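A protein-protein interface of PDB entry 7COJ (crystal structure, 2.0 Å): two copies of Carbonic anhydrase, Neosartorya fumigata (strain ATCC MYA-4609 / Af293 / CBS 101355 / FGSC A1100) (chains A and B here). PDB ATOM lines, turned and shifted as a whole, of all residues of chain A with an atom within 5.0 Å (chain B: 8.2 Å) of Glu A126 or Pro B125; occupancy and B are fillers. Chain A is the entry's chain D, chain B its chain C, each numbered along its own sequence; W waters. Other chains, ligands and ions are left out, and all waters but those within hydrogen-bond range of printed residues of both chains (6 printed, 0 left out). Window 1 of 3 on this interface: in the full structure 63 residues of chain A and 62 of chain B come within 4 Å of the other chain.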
ATOM      1  N   TRP A 116      10.696 -17.677   0.623  1.00  0.00           N
ATOM      2  CA  TRP A 116      10.999 -18.982   1.235  1.00  0.00           C
ATOM      3  C   TRP A 116      11.962 -18.806   2.406  1.00  0.00           C
ATOM      4  O   TRP A 116      13.021 -18.251   2.225  1.00  0.00           O
ATOM      5  CB  TRP A 116      11.583 -19.901   0.171  1.00  0.00           C
ATOM      6  CG  TRP A 116      12.080 -21.232   0.630  1.00  0.00           C
ATOM      7  CD1 TRP A 116      13.253 -21.511   1.261  1.00  0.00           C
ATOM      8  CD2 TRP A 116      11.426 -22.492   0.441  1.00  0.00           C
ATOM      9  NE1 TRP A 116      13.369 -22.850   1.481  1.00  0.00           N
ATOM     10  CE2 TRP A 116      12.270 -23.479   0.980  1.00  0.00           C
ATOM     11  CE3 TRP A 116      10.229 -22.886  -0.157  1.00  0.00           C
ATOM     12  CZ2 TRP A 116      11.933 -24.824   0.961  1.00  0.00           C
ATOM     13  CZ3 TRP A 116       9.895 -24.218  -0.169  1.00  0.00           C
ATOM     14  CH2 TRP A 116      10.737 -25.167   0.391  1.00  0.00           C
ATOM     15  N   CYS A 124      18.385 -28.953   0.978  1.00  0.00           N
ATOM     16  CA  CYS A 124      17.115 -28.193   0.805  1.00  0.00           C
ATOM     17  C   CYS A 124      17.288 -26.942  -0.056  1.00  0.00           C
ATOM     18  O   CYS A 124      16.859 -25.855   0.346  1.00  0.00           O
ATOM     19  CB  CYS A 124      16.577 -27.782   2.166  1.00  0.00           C
ATOM     20  SG  CYS A 124      16.440 -29.169   3.310  1.00  0.00           S
ATOM     21  N   PRO A 125      17.811 -27.036  -1.306  1.00  0.00           N
ATOM     22  CA  PRO A 125      17.795 -25.897  -2.232  1.00  0.00           C
ATOM     23  C   PRO A 125      16.406 -25.630  -2.850  1.00  0.00           C
ATOM     24  O   PRO A 125      15.923 -26.425  -3.668  1.00  0.00           O
ATOM     25  CB  PRO A 125      18.779 -26.306  -3.314  1.00  0.00           C
ATOM     26  CG  PRO A 125      18.690 -27.802  -3.336  1.00  0.00           C
ATOM     27  CD  PRO A 125      18.427 -28.227  -1.905  1.00  0.00           C
ATOM     28  N   GLU A 126      15.790 -24.536  -2.423  1.00  0.00           N
ATOM     29  CA  GLU A 126      14.354 -24.202  -2.633  1.00  0.00           C
ATOM     30  C   GLU A 126      14.029 -24.221  -4.127  1.00  0.00           C
ATOM     31  O   GLU A 126      13.010 -24.857  -4.512  1.00  0.00           O
ATOM     32  CB  GLU A 126      13.963 -22.876  -1.959  1.00  0.00           C
ATOM     33  CG  GLU A 126      14.530 -21.630  -2.607  1.00  0.00           C
ATOM     34  CD  GLU A 126      16.036 -21.584  -2.750  1.00  0.00           C
ATOM     35  OE1 GLU A 126      16.721 -21.890  -1.765  1.00  0.00           O
ATOM     36  OE2 GLU A 126      16.514 -21.242  -3.864  1.00  0.00           O
ATOM     37  N   THR A 127      14.835 -23.588  -4.965  1.00  0.00           N
ATOM     38  CA  THR A 127      14.480 -23.362  -6.376  1.00  0.00           C
ATOM     39  C   THR A 127      14.531 -24.705  -7.116  1.00  0.00           C
ATOM     40  O   THR A 127      13.653 -24.955  -7.952  1.00  0.00           O
ATOM     41  CB  THR A 127      15.363 -22.270  -6.989  1.00  0.00           C
ATOM     42  OG1 THR A 127      15.139 -21.068  -6.249  1.00  0.00           O
ATOM     43  CG2 THR A 127      15.032 -22.019  -8.439  1.00  0.00           C
ATOM     44  N   THR A 128      15.495 -25.555  -6.785  1.00  0.00           N
ATOM     45  CA  THR A 128      15.636 -26.918  -7.338  1.00  0.00           C
ATOM     46  C   THR A 128      14.416 -27.751  -6.912  1.00  0.00           C
ATOM     47  O   THR A 128      13.803 -28.357  -7.801  1.00  0.00           O
ATOM     48  CB  THR A 128      16.940 -27.587  -6.889  1.00  0.00           C
ATOM     49  OG1 THR A 128      18.015 -26.767  -7.363  1.00  0.00           O
ATOM     50  CG2 THR A 128      17.080 -29.014  -7.385  1.00  0.00           C
ATOM     51  N   ILE A 129      14.083 -27.817  -5.618  1.00  0.00           N
ATOM     52  CA  ILE A 129      13.081 -28.817  -5.141  1.00  0.00           C
ATOM     53  C   ILE A 129      11.671 -28.360  -5.541  1.00  0.00           C
ATOM     54  O   ILE A 129      10.766 -29.218  -5.590  1.00  0.00           O
ATOM     55  CB  ILE A 129      13.218 -29.132  -3.638  1.00  0.00           C
ATOM     56  CG1 ILE A 129      12.706 -28.007  -2.753  1.00  0.00           C
ATOM     57  CG2 ILE A 129      14.635 -29.550  -3.285  1.00  0.00           C
ATOM     58  CD1 ILE A 129      12.975 -28.222  -1.278  1.00  0.00           C
ATOM     59  N   LEU A 130      11.477 -27.066  -5.819  1.00  0.00           N
ATOM     60  CA  LEU A 130      10.185 -26.511  -6.299  1.00  0.00           C
ATOM     61  C   LEU A 130      10.069 -26.602  -7.829  1.00  0.00           C
ATOM     62  O   LEU A 130       8.980 -26.241  -8.364  1.00  0.00           O
ATOM     63  CB  LEU A 130      10.020 -25.078  -5.812  1.00  0.00           C
ATOM     64  CG  LEU A 130       9.842 -24.907  -4.296  1.00  0.00           C
ATOM     65  CD1 LEU A 130       9.836 -23.428  -3.931  1.00  0.00           C
ATOM     66  CD2 LEU A 130       8.543 -25.549  -3.813  1.00  0.00           C
ATOM     67  N   GLY A 131      11.119 -27.042  -8.515  1.00  0.00           N
ATOM     68  CA  GLY A 131      11.137 -27.104  -9.994  1.00  0.00           C
ATOM     69  C   GLY A 131      10.960 -25.722 -10.591  1.00  0.00           C
ATOM     70  O   GLY A 131      10.272 -25.616 -11.619  1.00  0.00           O
ATOM     71  N   PRO A 134      15.476 -19.158 -11.438  1.00  0.00           N
ATOM     72  CA  PRO A 134      15.908 -17.889 -10.888  1.00  0.00           C
ATOM     73  C   PRO A 134      14.812 -16.845 -11.145  1.00  0.00           C
ATOM     74  O   PRO A 134      14.213 -16.881 -12.204  1.00  0.00           O
ATOM     75  CB  PRO A 134      17.163 -17.580 -11.697  1.00  0.00           C
ATOM     76  CG  PRO A 134      17.696 -18.923 -12.122  1.00  0.00           C
ATOM     77  CD  PRO A 134      16.460 -19.745 -12.372  1.00  0.00           C
ATOM     78  N   VAL A 137      11.824 -17.297  -6.430  1.00  0.00           N
ATOM     79  CA  VAL A 137      11.756 -17.522  -4.963  1.00  0.00           C
ATOM     80  C   VAL A 137      12.747 -16.606  -4.256  1.00  0.00           C
ATOM     81  O   VAL A 137      13.960 -16.837  -4.353  1.00  0.00           O
ATOM     82  CB  VAL A 137      11.999 -19.000  -4.626  1.00  0.00           C
ATOM     83  CG1 VAL A 137      11.808 -19.254  -3.148  1.00  0.00           C
ATOM     84  CG2 VAL A 137      11.115 -19.928  -5.448  1.00  0.00           C
ATOM     85  N   THR A 139      14.638 -15.786  -1.049  1.00  0.00           N
ATOM     86  CA  THR A 139      15.098 -16.884  -0.161  1.00  0.00           C
ATOM     87  C   THR A 139      15.881 -16.393   1.055  1.00  0.00           C
ATOM     88  O   THR A 139      16.897 -15.663   0.901  1.00  0.00           O
ATOM     89  CB  THR A 139      15.955 -17.888  -0.942  1.00  0.00           C
ATOM     90  OG1 THR A 139      15.147 -18.384  -2.011  1.00  0.00           O
ATOM     91  CG2 THR A 139      16.430 -19.029  -0.076  1.00  0.00           C
ATOM     92  N   ARG A 141      17.758 -18.665   4.251  1.00  0.00           N
ATOM     93  CA  ARG A 141      18.079 -19.994   4.825  1.00  0.00           C
ATOM     94  C   ARG A 141      19.003 -19.779   6.029  1.00  0.00           C
ATOM     95  O   ARG A 141      20.012 -19.019   5.922  1.00  0.00           O
ATOM     96  CB  ARG A 141      18.639 -20.915   3.742  1.00  0.00           C
ATOM     97  CG  ARG A 141      17.599 -21.361   2.718  1.00  0.00           C
ATOM     98  CD  ARG A 141      18.198 -22.003   1.496  1.00  0.00           C
ATOM     99  NE  ARG A 141      18.805 -23.290   1.769  1.00  0.00           N
ATOM    100  CZ  ARG A 141      19.537 -23.978   0.891  1.00  0.00           C
ATOM    101  NH1 ARG A 141      19.744 -23.516  -0.337  1.00  0.00           N
ATOM    102  NH2 ARG A 141      20.061 -25.133   1.258  1.00  0.00           N
ATOM    103  N   ALA B  84       3.686 -24.468  -7.370  1.00  0.00           N
ATOM    104  CA  ALA B  84       5.033 -24.862  -6.907  1.00  0.00           C
ATOM    105  C   ALA B  84       4.984 -26.250  -6.291  1.00  0.00           C
ATOM    106  O   ALA B  84       5.915 -27.015  -6.537  1.00  0.00           O
ATOM    107  CB  ALA B  84       5.588 -23.840  -5.938  1.00  0.00           C
ATOM    108  N   ASN B  88       7.058 -29.435  -7.510  1.00  0.00           N
ATOM    109  CA  ASN B  88       7.859 -30.241  -6.567  1.00  0.00           C
ATOM    110  C   ASN B  88       7.587 -31.736  -6.822  1.00  0.00           C
ATOM    111  O   ASN B  88       8.534 -32.513  -6.879  1.00  0.00           O
ATOM    112  CB  ASN B  88       7.584 -29.871  -5.110  1.00  0.00           C
ATOM    113  CG  ASN B  88       8.118 -30.917  -4.147  1.00  0.00           C
ATOM    114  OD1 ASN B  88       9.351 -31.119  -4.042  1.00  0.00           O
ATOM    115  ND2 ASN B  88       7.200 -31.623  -3.500  1.00  0.00           N
ATOM    116  N   TRP B  91       9.274 -32.799  -9.920  1.00  0.00           N
ATOM    117  CA  TRP B  91      10.734 -32.903  -9.686  1.00  0.00           C
ATOM    118  C   TRP B  91      11.061 -34.183  -8.901  1.00  0.00           C
ATOM    119  O   TRP B  91      11.997 -34.893  -9.275  1.00  0.00           O
ATOM    120  CB  TRP B  91      11.259 -31.629  -9.019  1.00  0.00           C
ATOM    121  CG  TRP B  91      12.701 -31.748  -8.659  1.00  0.00           C
ATOM    122  CD1 TRP B  91      13.790 -31.572  -9.460  1.00  0.00           C
ATOM    123  CD2 TRP B  91      13.198 -32.138  -7.375  1.00  0.00           C
ATOM    124  NE1 TRP B  91      14.943 -31.809  -8.741  1.00  0.00           N
ATOM    125  CE2 TRP B  91      14.610 -32.089  -7.449  1.00  0.00           C
ATOM    126  CE3 TRP B  91      12.587 -32.434  -6.156  1.00  0.00           C
ATOM    127  CZ2 TRP B  91      15.414 -32.395  -6.357  1.00  0.00           C
ATOM    128  CZ3 TRP B  91      13.386 -32.708  -5.074  1.00  0.00           C
ATOM    129  CH2 TRP B  91      14.775 -32.700  -5.177  1.00  0.00           C
ATOM    130  N   TRP B 116      28.029 -21.450   0.945  1.00  0.00           N
ATOM    131  CA  TRP B 116      27.654 -20.268   0.144  1.00  0.00           C
ATOM    132  C   TRP B 116      26.932 -19.275   1.054  1.00  0.00           C
ATOM    133  O   TRP B 116      25.901 -19.652   1.677  1.00  0.00           O
ATOM    134  CB  TRP B 116      26.769 -20.723  -0.995  1.00  0.00           C
ATOM    135  CG  TRP B 116      26.230 -19.642  -1.877  1.00  0.00           C
ATOM    136  CD1 TRP B 116      25.126 -18.868  -1.662  1.00  0.00           C
ATOM    137  CD2 TRP B 116      26.703 -19.323  -3.183  1.00  0.00           C
ATOM    138  NE1 TRP B 116      24.910 -18.057  -2.736  1.00  0.00           N
ATOM    139  CE2 TRP B 116      25.858 -18.325  -3.686  1.00  0.00           C
ATOM    140  CE3 TRP B 116      27.752 -19.787  -3.973  1.00  0.00           C
ATOM    141  CZ2 TRP B 116      26.028 -17.787  -4.952  1.00  0.00           C
ATOM    142  CZ3 TRP B 116      27.927 -19.246  -5.223  1.00  0.00           C
ATOM    143  CH2 TRP B 116      27.083 -18.263  -5.697  1.00  0.00           C
ATOM    144  N   CYS B 119      23.077 -13.311  -1.478  1.00  0.00           N
ATOM    145  CA  CYS B 119      21.919 -12.429  -1.313  1.00  0.00           C
ATOM    146  C   CYS B 119      20.644 -13.285  -1.416  1.00  0.00           C
ATOM    147  O   CYS B 119      20.597 -14.276  -2.196  1.00  0.00           O
ATOM    148  CB  CYS B 119      21.946 -11.278  -2.306  1.00  0.00           C
ATOM    149  SG  CYS B 119      20.643 -10.165  -1.934  1.00  0.00           S
ATOM    150  N   SER B 120      19.628 -12.876  -0.670  1.00  0.00           N
ATOM    151  CA  SER B 120      18.247 -13.423  -0.733  1.00  0.00           C
ATOM    152  C   SER B 120      17.607 -13.177  -2.106  1.00  0.00           C
ATOM    153  O   SER B 120      16.606 -13.802  -2.421  1.00  0.00           O
ATOM    154  CB  SER B 120      17.452 -12.810   0.376  1.00  0.00           C
ATOM    155  OG  SER B 120      17.954 -13.272   1.619  1.00  0.00           O
ATOM    156  N   ASP B 121      18.139 -12.241  -2.884  1.00  0.00           N
ATOM    157  CA  ASP B 121      17.614 -11.879  -4.232  1.00  0.00           C
ATOM    158  C   ASP B 121      17.178 -13.156  -4.963  1.00  0.00           C
ATOM    159  O   ASP B 121      17.986 -14.104  -5.070  1.00  0.00           O
ATOM    160  CB  ASP B 121      18.653 -11.073  -5.022  1.00  0.00           C
ATOM    161  CG  ASP B 121      18.107 -10.411  -6.276  1.00  0.00           C
ATOM    162  OD1 ASP B 121      17.655 -11.146  -7.216  1.00  0.00           O
ATOM    163  OD2 ASP B 121      18.136  -9.173  -6.306  1.00  0.00           O
ATOM    164  N   SER B 122      15.946 -13.184  -5.460  1.00  0.00           N
ATOM    165  CA  SER B 122      15.322 -14.354  -6.123  1.00  0.00           C
ATOM    166  C   SER B 122      16.133 -14.748  -7.352  1.00  0.00           C
ATOM    167  O   SER B 122      16.000 -15.903  -7.787  1.00  0.00           O
ATOM    168  CB  SER B 122      13.898 -14.082  -6.518  1.00  0.00           C
ATOM    169  OG  SER B 122      13.831 -12.983  -7.417  1.00  0.00           O
ATOM    170  N   ARG B 123      16.951 -13.857  -7.896  1.00  0.00           N
ATOM    171  CA  ARG B 123      17.752 -14.162  -9.107  1.00  0.00           C
ATOM    172  C   ARG B 123      19.055 -14.907  -8.764  1.00  0.00           C
ATOM    173  O   ARG B 123      19.732 -15.276  -9.725  1.00  0.00           O
ATOM    174  CB  ARG B 123      18.036 -12.879  -9.882  1.00  0.00           C
ATOM    175  CG  ARG B 123      16.777 -12.169 -10.334  1.00  0.00           C
ATOM    176  CD  ARG B 123      17.021 -10.755 -10.839  1.00  0.00           C
ATOM    177  NE  ARG B 123      17.368  -9.882  -9.738  1.00  0.00           N
ATOM    178  CZ  ARG B 123      17.612  -8.579  -9.842  1.00  0.00           C
ATOM    179  NH1 ARG B 123      17.493  -7.965 -11.014  1.00  0.00           N
ATOM    180  NH2 ARG B 123      17.966  -7.895  -8.774  1.00  0.00           N
ATOM    181  N   CYS B 124      19.384 -15.172  -7.489  1.00  0.00           N
ATOM    182  CA  CYS B 124      20.688 -15.811  -7.110  1.00  0.00           C
ATOM    183  C   CYS B 124      20.509 -17.126  -6.353  1.00  0.00           C
ATOM    184  O   CYS B 124      21.086 -17.314  -5.280  1.00  0.00           O
ATOM    185  CB  CYS B 124      21.589 -14.880  -6.300  1.00  0.00           C
ATOM    186  SG  CYS B 124      23.361 -15.264  -6.493  1.00  0.00           S
ATOM    187  N   PRO B 125      19.793 -18.130  -6.911  1.00  0.00           N
ATOM    188  CA  PRO B 125      19.742 -19.467  -6.310  1.00  0.00           C
ATOM    189  C   PRO B 125      21.009 -20.301  -6.555  1.00  0.00           C
ATOM    190  O   PRO B 125      21.255 -20.731  -7.680  1.00  0.00           O
ATOM    191  CB  PRO B 125      18.543 -20.137  -6.981  1.00  0.00           C
ATOM    192  CG  PRO B 125      18.496 -19.464  -8.346  1.00  0.00           C
ATOM    193  CD  PRO B 125      18.939 -18.045  -8.107  1.00  0.00           C
ATOM    194  N   GLU B 126      21.783 -20.502  -5.492  1.00  0.00           N
ATOM    195  CA  GLU B 126      23.194 -20.971  -5.528  1.00  0.00           C
ATOM    196  C   GLU B 126      23.282 -22.313  -6.281  1.00  0.00           C
ATOM    197  O   GLU B 126      24.175 -22.465  -7.159  1.00  0.00           O
ATOM    198  CB  GLU B 126      23.803 -21.011  -4.128  1.00  0.00           C
ATOM    199  CG  GLU B 126      23.308 -22.141  -3.247  1.00  0.00           C
ATOM    200  CD  GLU B 126      21.803 -22.166  -3.023  1.00  0.00           C
ATOM    201  OE1 GLU B 126      21.225 -21.083  -2.718  1.00  0.00           O
ATOM    202  OE2 GLU B 126      21.210 -23.253  -3.154  1.00  0.00           O
ATOM    203  N   THR B 127      22.417 -23.269  -5.977  1.00  0.00           N
ATOM    204  CA  THR B 127      22.564 -24.651  -6.484  1.00  0.00           C
ATOM    205  C   THR B 127      22.273 -24.658  -7.983  1.00  0.00           C
ATOM    206  O   THR B 127      22.994 -25.343  -8.721  1.00  0.00           O
ATOM    207  CB  THR B 127      21.700 -25.627  -5.682  1.00  0.00           C
ATOM    208  OG1 THR B 127      22.176 -25.572  -4.345  1.00  0.00           O
ATOM    209  CG2 THR B 127      21.786 -27.051  -6.199  1.00  0.00           C
ATOM    210  N   THR B 128      21.290 -23.878  -8.425  1.00  0.00           N
ATOM    211  CA  THR B 128      20.929 -23.707  -9.842  1.00  0.00           C
ATOM    212  C   THR B 128      22.118 -23.058 -10.572  1.00  0.00           C
ATOM    213  O   THR B 128      22.515 -23.605 -11.620  1.00  0.00           O
ATOM    214  CB  THR B 128      19.659 -22.873 -10.027  1.00  0.00           C
ATOM    215  OG1 THR B 128      18.607 -23.556  -9.344  1.00  0.00           O
ATOM    216  CG2 THR B 128      19.316 -22.668 -11.486  1.00  0.00           C
ATOM    217  N   ILE B 129      22.653 -21.936 -10.081  1.00  0.00           N
ATOM    218  CA  ILE B 129      23.596 -21.123 -10.900  1.00  0.00           C
ATOM    219  C   ILE B 129      24.968 -21.808 -10.918  1.00  0.00           C
ATOM    220  O   ILE B 129      25.757 -21.517 -11.846  1.00  0.00           O
ATOM    221  CB  ILE B 129      23.640 -19.650 -10.470  1.00  0.00           C
ATOM    222  CG1 ILE B 129      24.415 -19.451  -9.173  1.00  0.00           C
ATOM    223  CG2 ILE B 129      22.239 -19.029 -10.442  1.00  0.00           C
ATOM    224  CD1 ILE B 129      24.285 -18.024  -8.626  1.00  0.00           C
ATOM    225  N   LEU B 130      25.262 -22.673  -9.950  1.00  0.00           N
ATOM    226  CA  LEU B 130      26.515 -23.477  -9.918  1.00  0.00           C
ATOM    227  C   LEU B 130      26.365 -24.795 -10.706  1.00  0.00           C
ATOM    228  O   LEU B 130      27.358 -25.537 -10.814  1.00  0.00           O
ATOM    229  CB  LEU B 130      26.943 -23.750  -8.483  1.00  0.00           C
ATOM    230  CG  LEU B 130      27.337 -22.525  -7.656  1.00  0.00           C
ATOM    231  CD1 LEU B 130      27.551 -22.904  -6.198  1.00  0.00           C
ATOM    232  CD2 LEU B 130      28.627 -21.922  -8.188  1.00  0.00           C
ATOM    233  N   GLY B 131      25.184 -25.073 -11.239  1.00  0.00           N
ATOM    234  CA  GLY B 131      24.877 -26.335 -11.943  1.00  0.00           C
ATOM    235  C   GLY B 131      25.085 -27.532 -11.042  1.00  0.00           C
ATOM    236  O   GLY B 131      25.567 -28.539 -11.549  1.00  0.00           O
ATOM    237  N   LEU B 132      24.728 -27.444  -9.755  1.00  0.00           N
ATOM    238  CA  LEU B 132      25.011 -28.523  -8.770  1.00  0.00           C
ATOM    239  C   LEU B 132      23.709 -29.182  -8.336  1.00  0.00           C
ATOM    240  O   LEU B 132      22.665 -28.873  -8.890  1.00  0.00           O
ATOM    241  CB  LEU B 132      25.814 -27.933  -7.606  1.00  0.00           C
ATOM    242  CG  LEU B 132      27.264 -27.590  -7.957  1.00  0.00           C
ATOM    243  CD1 LEU B 132      27.979 -26.916  -6.790  1.00  0.00           C
ATOM    244  CD2 LEU B 132      28.027 -28.823  -8.405  1.00  0.00           C
ATOM    245  N   PRO B 134      21.225 -31.043  -4.948  1.00  0.00           N
ATOM    246  CA  PRO B 134      21.022 -31.075  -3.508  1.00  0.00           C
ATOM    247  C   PRO B 134      22.179 -31.853  -2.880  1.00  0.00           C
ATOM    248  O   PRO B 134      22.617 -32.844  -3.474  1.00  0.00           O
ATOM    249  CB  PRO B 134      19.699 -31.820  -3.343  1.00  0.00           C
ATOM    250  CG  PRO B 134      18.993 -31.615  -4.665  1.00  0.00           C
ATOM    251  CD  PRO B 134      20.077 -31.535  -5.723  1.00  0.00           C
ATOM    252  N   VAL B 137      25.798 -27.754  -1.649  1.00  0.00           N
ATOM    253  CA  VAL B 137      26.062 -26.373  -1.179  1.00  0.00           C
ATOM    254  C   VAL B 137      25.294 -26.085   0.117  1.00  0.00           C
ATOM    255  O   VAL B 137      24.070 -25.937   0.059  1.00  0.00           O
ATOM    256  CB  VAL B 137      25.728 -25.366  -2.290  1.00  0.00           C
ATOM    257  CG1 VAL B 137      26.142 -23.966  -1.869  1.00  0.00           C
ATOM    258  CG2 VAL B 137      26.369 -25.746  -3.621  1.00  0.00           C
ATOM    259  N   THR B 139      24.019 -23.481   2.597  1.00  0.00           N
ATOM    260  CA  THR B 139      23.598 -22.141   2.096  1.00  0.00           C
ATOM    261  C   THR B 139      23.056 -21.217   3.194  1.00  0.00           C
ATOM    262  O   THR B 139      22.094 -21.590   3.923  1.00  0.00           O
ATOM    263  CB  THR B 139      22.544 -22.265   1.007  1.00  0.00           C
ATOM    264  OG1 THR B 139      23.101 -23.079  -0.025  1.00  0.00           O
ATOM    265  CG2 THR B 139      22.121 -20.916   0.464  1.00  0.00           C
ATOM    266  N   ARG B 141      21.549 -17.179   2.940  1.00  0.00           N
ATOM    267  CA  ARG B 141      21.182 -16.025   2.077  1.00  0.00           C
ATOM    268  C   ARG B 141      20.468 -14.986   2.941  1.00  0.00           C
ATOM    269  O   ARG B 141      19.564 -15.373   3.721  1.00  0.00           O
ATOM    270  CB  ARG B 141      20.375 -16.483   0.865  1.00  0.00           C
ATOM    271  CG  ARG B 141      21.167 -17.279  -0.151  1.00  0.00           C
ATOM    272  CD  ARG B 141      20.300 -17.975  -1.159  1.00  0.00           C
ATOM    273  NE  ARG B 141      19.625 -17.061  -2.053  1.00  0.00           N
ATOM    274  CZ  ARG B 141      18.715 -17.426  -2.958  1.00  0.00           C
ATOM    275  NH1 ARG B 141      18.348 -18.692  -3.080  1.00  0.00           N
ATOM    276  NH2 ARG B 141      18.177 -16.509  -3.733  1.00  0.00           N
ATOM    277  N   TYR B 257      27.974 -12.333  -8.865  1.00  0.00           N
ATOM    278  CA  TYR B 257      27.046 -12.939  -9.832  1.00  0.00           C
ATOM    279  C   TYR B 257      26.470 -11.833 -10.712  1.00  0.00           C
ATOM    280  O   TYR B 257      25.906 -10.854 -10.201  1.00  0.00           O
ATOM    281  CB  TYR B 257      25.945 -13.706  -9.115  1.00  0.00           C
ATOM    282  CG  TYR B 257      24.974 -14.359 -10.046  1.00  0.00           C
ATOM    283  CD1 TYR B 257      25.403 -15.341 -10.918  1.00  0.00           C
ATOM    284  CD2 TYR B 257      23.654 -13.953 -10.102  1.00  0.00           C
ATOM    285  CE1 TYR B 257      24.518 -15.953 -11.788  1.00  0.00           C
ATOM    286  CE2 TYR B 257      22.756 -14.552 -10.964  1.00  0.00           C
ATOM    287  CZ  TYR B 257      23.195 -15.560 -11.813  1.00  0.00           C
ATOM    288  OH  TYR B 257      22.333 -16.153 -12.677  1.00  0.00           O
ATOM    289  N   VAL B 259      23.528 -10.945 -12.830  1.00  0.00           N
ATOM    290  CA  VAL B 259      22.122 -11.421 -12.965  1.00  0.00           C
ATOM    291  C   VAL B 259      21.701 -11.372 -14.442  1.00  0.00           C
ATOM    292  O   VAL B 259      20.746 -12.069 -14.779  1.00  0.00           O
ATOM    293  CB  VAL B 259      21.139 -10.645 -12.068  1.00  0.00           C
ATOM    294  CG1 VAL B 259      21.470 -10.867 -10.598  1.00  0.00           C
ATOM    295  CG2 VAL B 259      21.102  -9.160 -12.418  1.00  0.00           C
HETATM  296  O   HOH W   1      19.072 -21.004  -1.505  1.00  0.00           O
HETATM  297  O   HOH W   2      14.261 -18.667  -7.619  1.00  0.00           O
HETATM  298  O   HOH W   3      21.527 -26.217  -1.079  1.00  0.00           O
HETATM  299  O   HOH W   4      16.225 -17.913  -5.476  1.00  0.00           O
HETATM  300  O   HOH W   5      18.788 -22.721  -4.528  1.00  0.00           O
HETATM  301  O   HOH W   6      18.511 -24.215  -6.738  1.00  0.00           O
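Water W6 bridges OG1 of Thr A128 and OG1 of Thr B128.
Water W4 lies within hydrogen-bond range of the backbone carbonyl oxygen of Val A137 (2.7 Å), the guanidinium group of Arg B141 (3.0 Å), the backbone carbonyl oxygen of Ser B122 (3.1 Å) and the side-chain hydroxyl of Thr A127 (3.4 Å).
Water W3 lies within hydrogen-bond range of the backbone carbonyl oxygen (O) of Val B137, the guanidinium group (NH2) of Arg A141 and the side-chain hydroxyl (OG1) of Thr B127.
Water W2 lies within hydrogen-bond range of OG1 of Thr A127 (2.9 Å), N of Val A137 (3.0 Å) and O of Ser B122 (3.3 Å).
Glu A126 touches two residues of chain B.
Of the printed residues of chain B, Ile A129 touches Asn B88 and Trp B91.
Printed residues of chain B within 4 Å of Pro A134: Ser B122, Arg B123 and Pro B125.
Printed residues of chain A within 4 Å of Trp B91: Thr A128 and Ile A129.
Of the printed residues of chain A, Ser B120 touches Thr A139 (2.7 Å).
Of chain A, only Glu A126 (3.9 Å), Thr A127 (3.6 Å) and Pro A134 (3.9 Å) come within 4 Å of Pro B125.
The nearest printed residue of chain A that does not touch Pro B125 is Thr A128 (6.2 Å).
The side-chain hydroxyl (OG1) of Thr A127 lies within hydrogen-bond range of the side-chain carboxylate (OE2) of Glu A126 (2.8 Å).
The guanidinium group of Arg B123 is in salt-bridge range of the side-chain carboxylate of Asp B121, at 2.8 Å.
O of Cys A124 sits close to NH2 of Arg A141.
NH2 of Arg B141 sits close to O of Cys B124.
O of Thr B127 sits at hydrogen-bond distance from N of Leu B132, at 2.9 Å.
The backbone carbonyl oxygen of Val B137 is in hydrogen-bond range of the side-chain hydroxyl of Thr B139, 3.0 Å away.
Of the 24 printed residues of chain B, 12 touch a printed residue of chain A.
Hydrophobic or aromatic side chains of chain B that line the printed part of chain A: Trp B91 and Pro B125.
Printed residues of chain A that touch a printed residue of chain B: Pro A125, Glu A126, Thr A127, Thr A128, Ile A129, Leu A130, Pro A134, Val A137, Thr A139 and Arg A141.
Hydrophobic or aromatic side chains of chain A within 4 Å of the printed part of chain B: Pro A125, Ile A129 and Pro A134.
Among the printed residues, 22 pairs touch across the chains.
The guanidinium group of Arg A141 is in salt-bridge range of the side-chain carboxylate of Glu B126, at 3.2 Å.
NH1 of Arg B141 is in salt-bridge range of OE2 of Glu A126 (3.2 Å).
The backbone carbonyl oxygen (O) of Ile A129 sits close to the side-chain amide oxygen (OD1) of Asn B88 (2.8 Å).
OG of Ser B120 lies within hydrogen-bond range of O of Thr A139, at 2.7 Å.
OG1 of Thr B139 sits close to NH1 of Arg A141, 3.4 Å away.
The side-chain hydroxyl of Thr A139 lies close to the guanidinium group of Arg B141.
Pro A125 touches Glu B126.
Glu A126 touches Pro B125.
Thr A127 touches Pro B125.
Thr A127 touches Thr B128 (CG2 to OG1, 3.995 Å).
Trp B91 touches Thr A128 (CD1 to O, 3.6 Å).
Thr A128 touches Thr B127.
Ala B84 touches Leu A130 (O to O, 3.7 Å).
Pro A134 touches Arg B123.
Pro A134 touches Pro B125 (CG to CG, 3.9 Å).
Arg B141 touches Arg A141.
Pro A125 touches Glu B126, and with the chains exchanged Glu A126 touches Pro B125.
Pro A125 touches Thr B127, and with the chains exchanged Thr A127 touches Pro B125.
Thr A127 touches Thr B128, and with the chains exchanged Thr A128 touches Thr B127.
Thr A128 touches its own counterpart, Thr B128.
13 positions are printed for both chains.
Of the 22 pairs that touch across the chains among the printed residues, 12 have their exchanged pair printed and touching as well.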
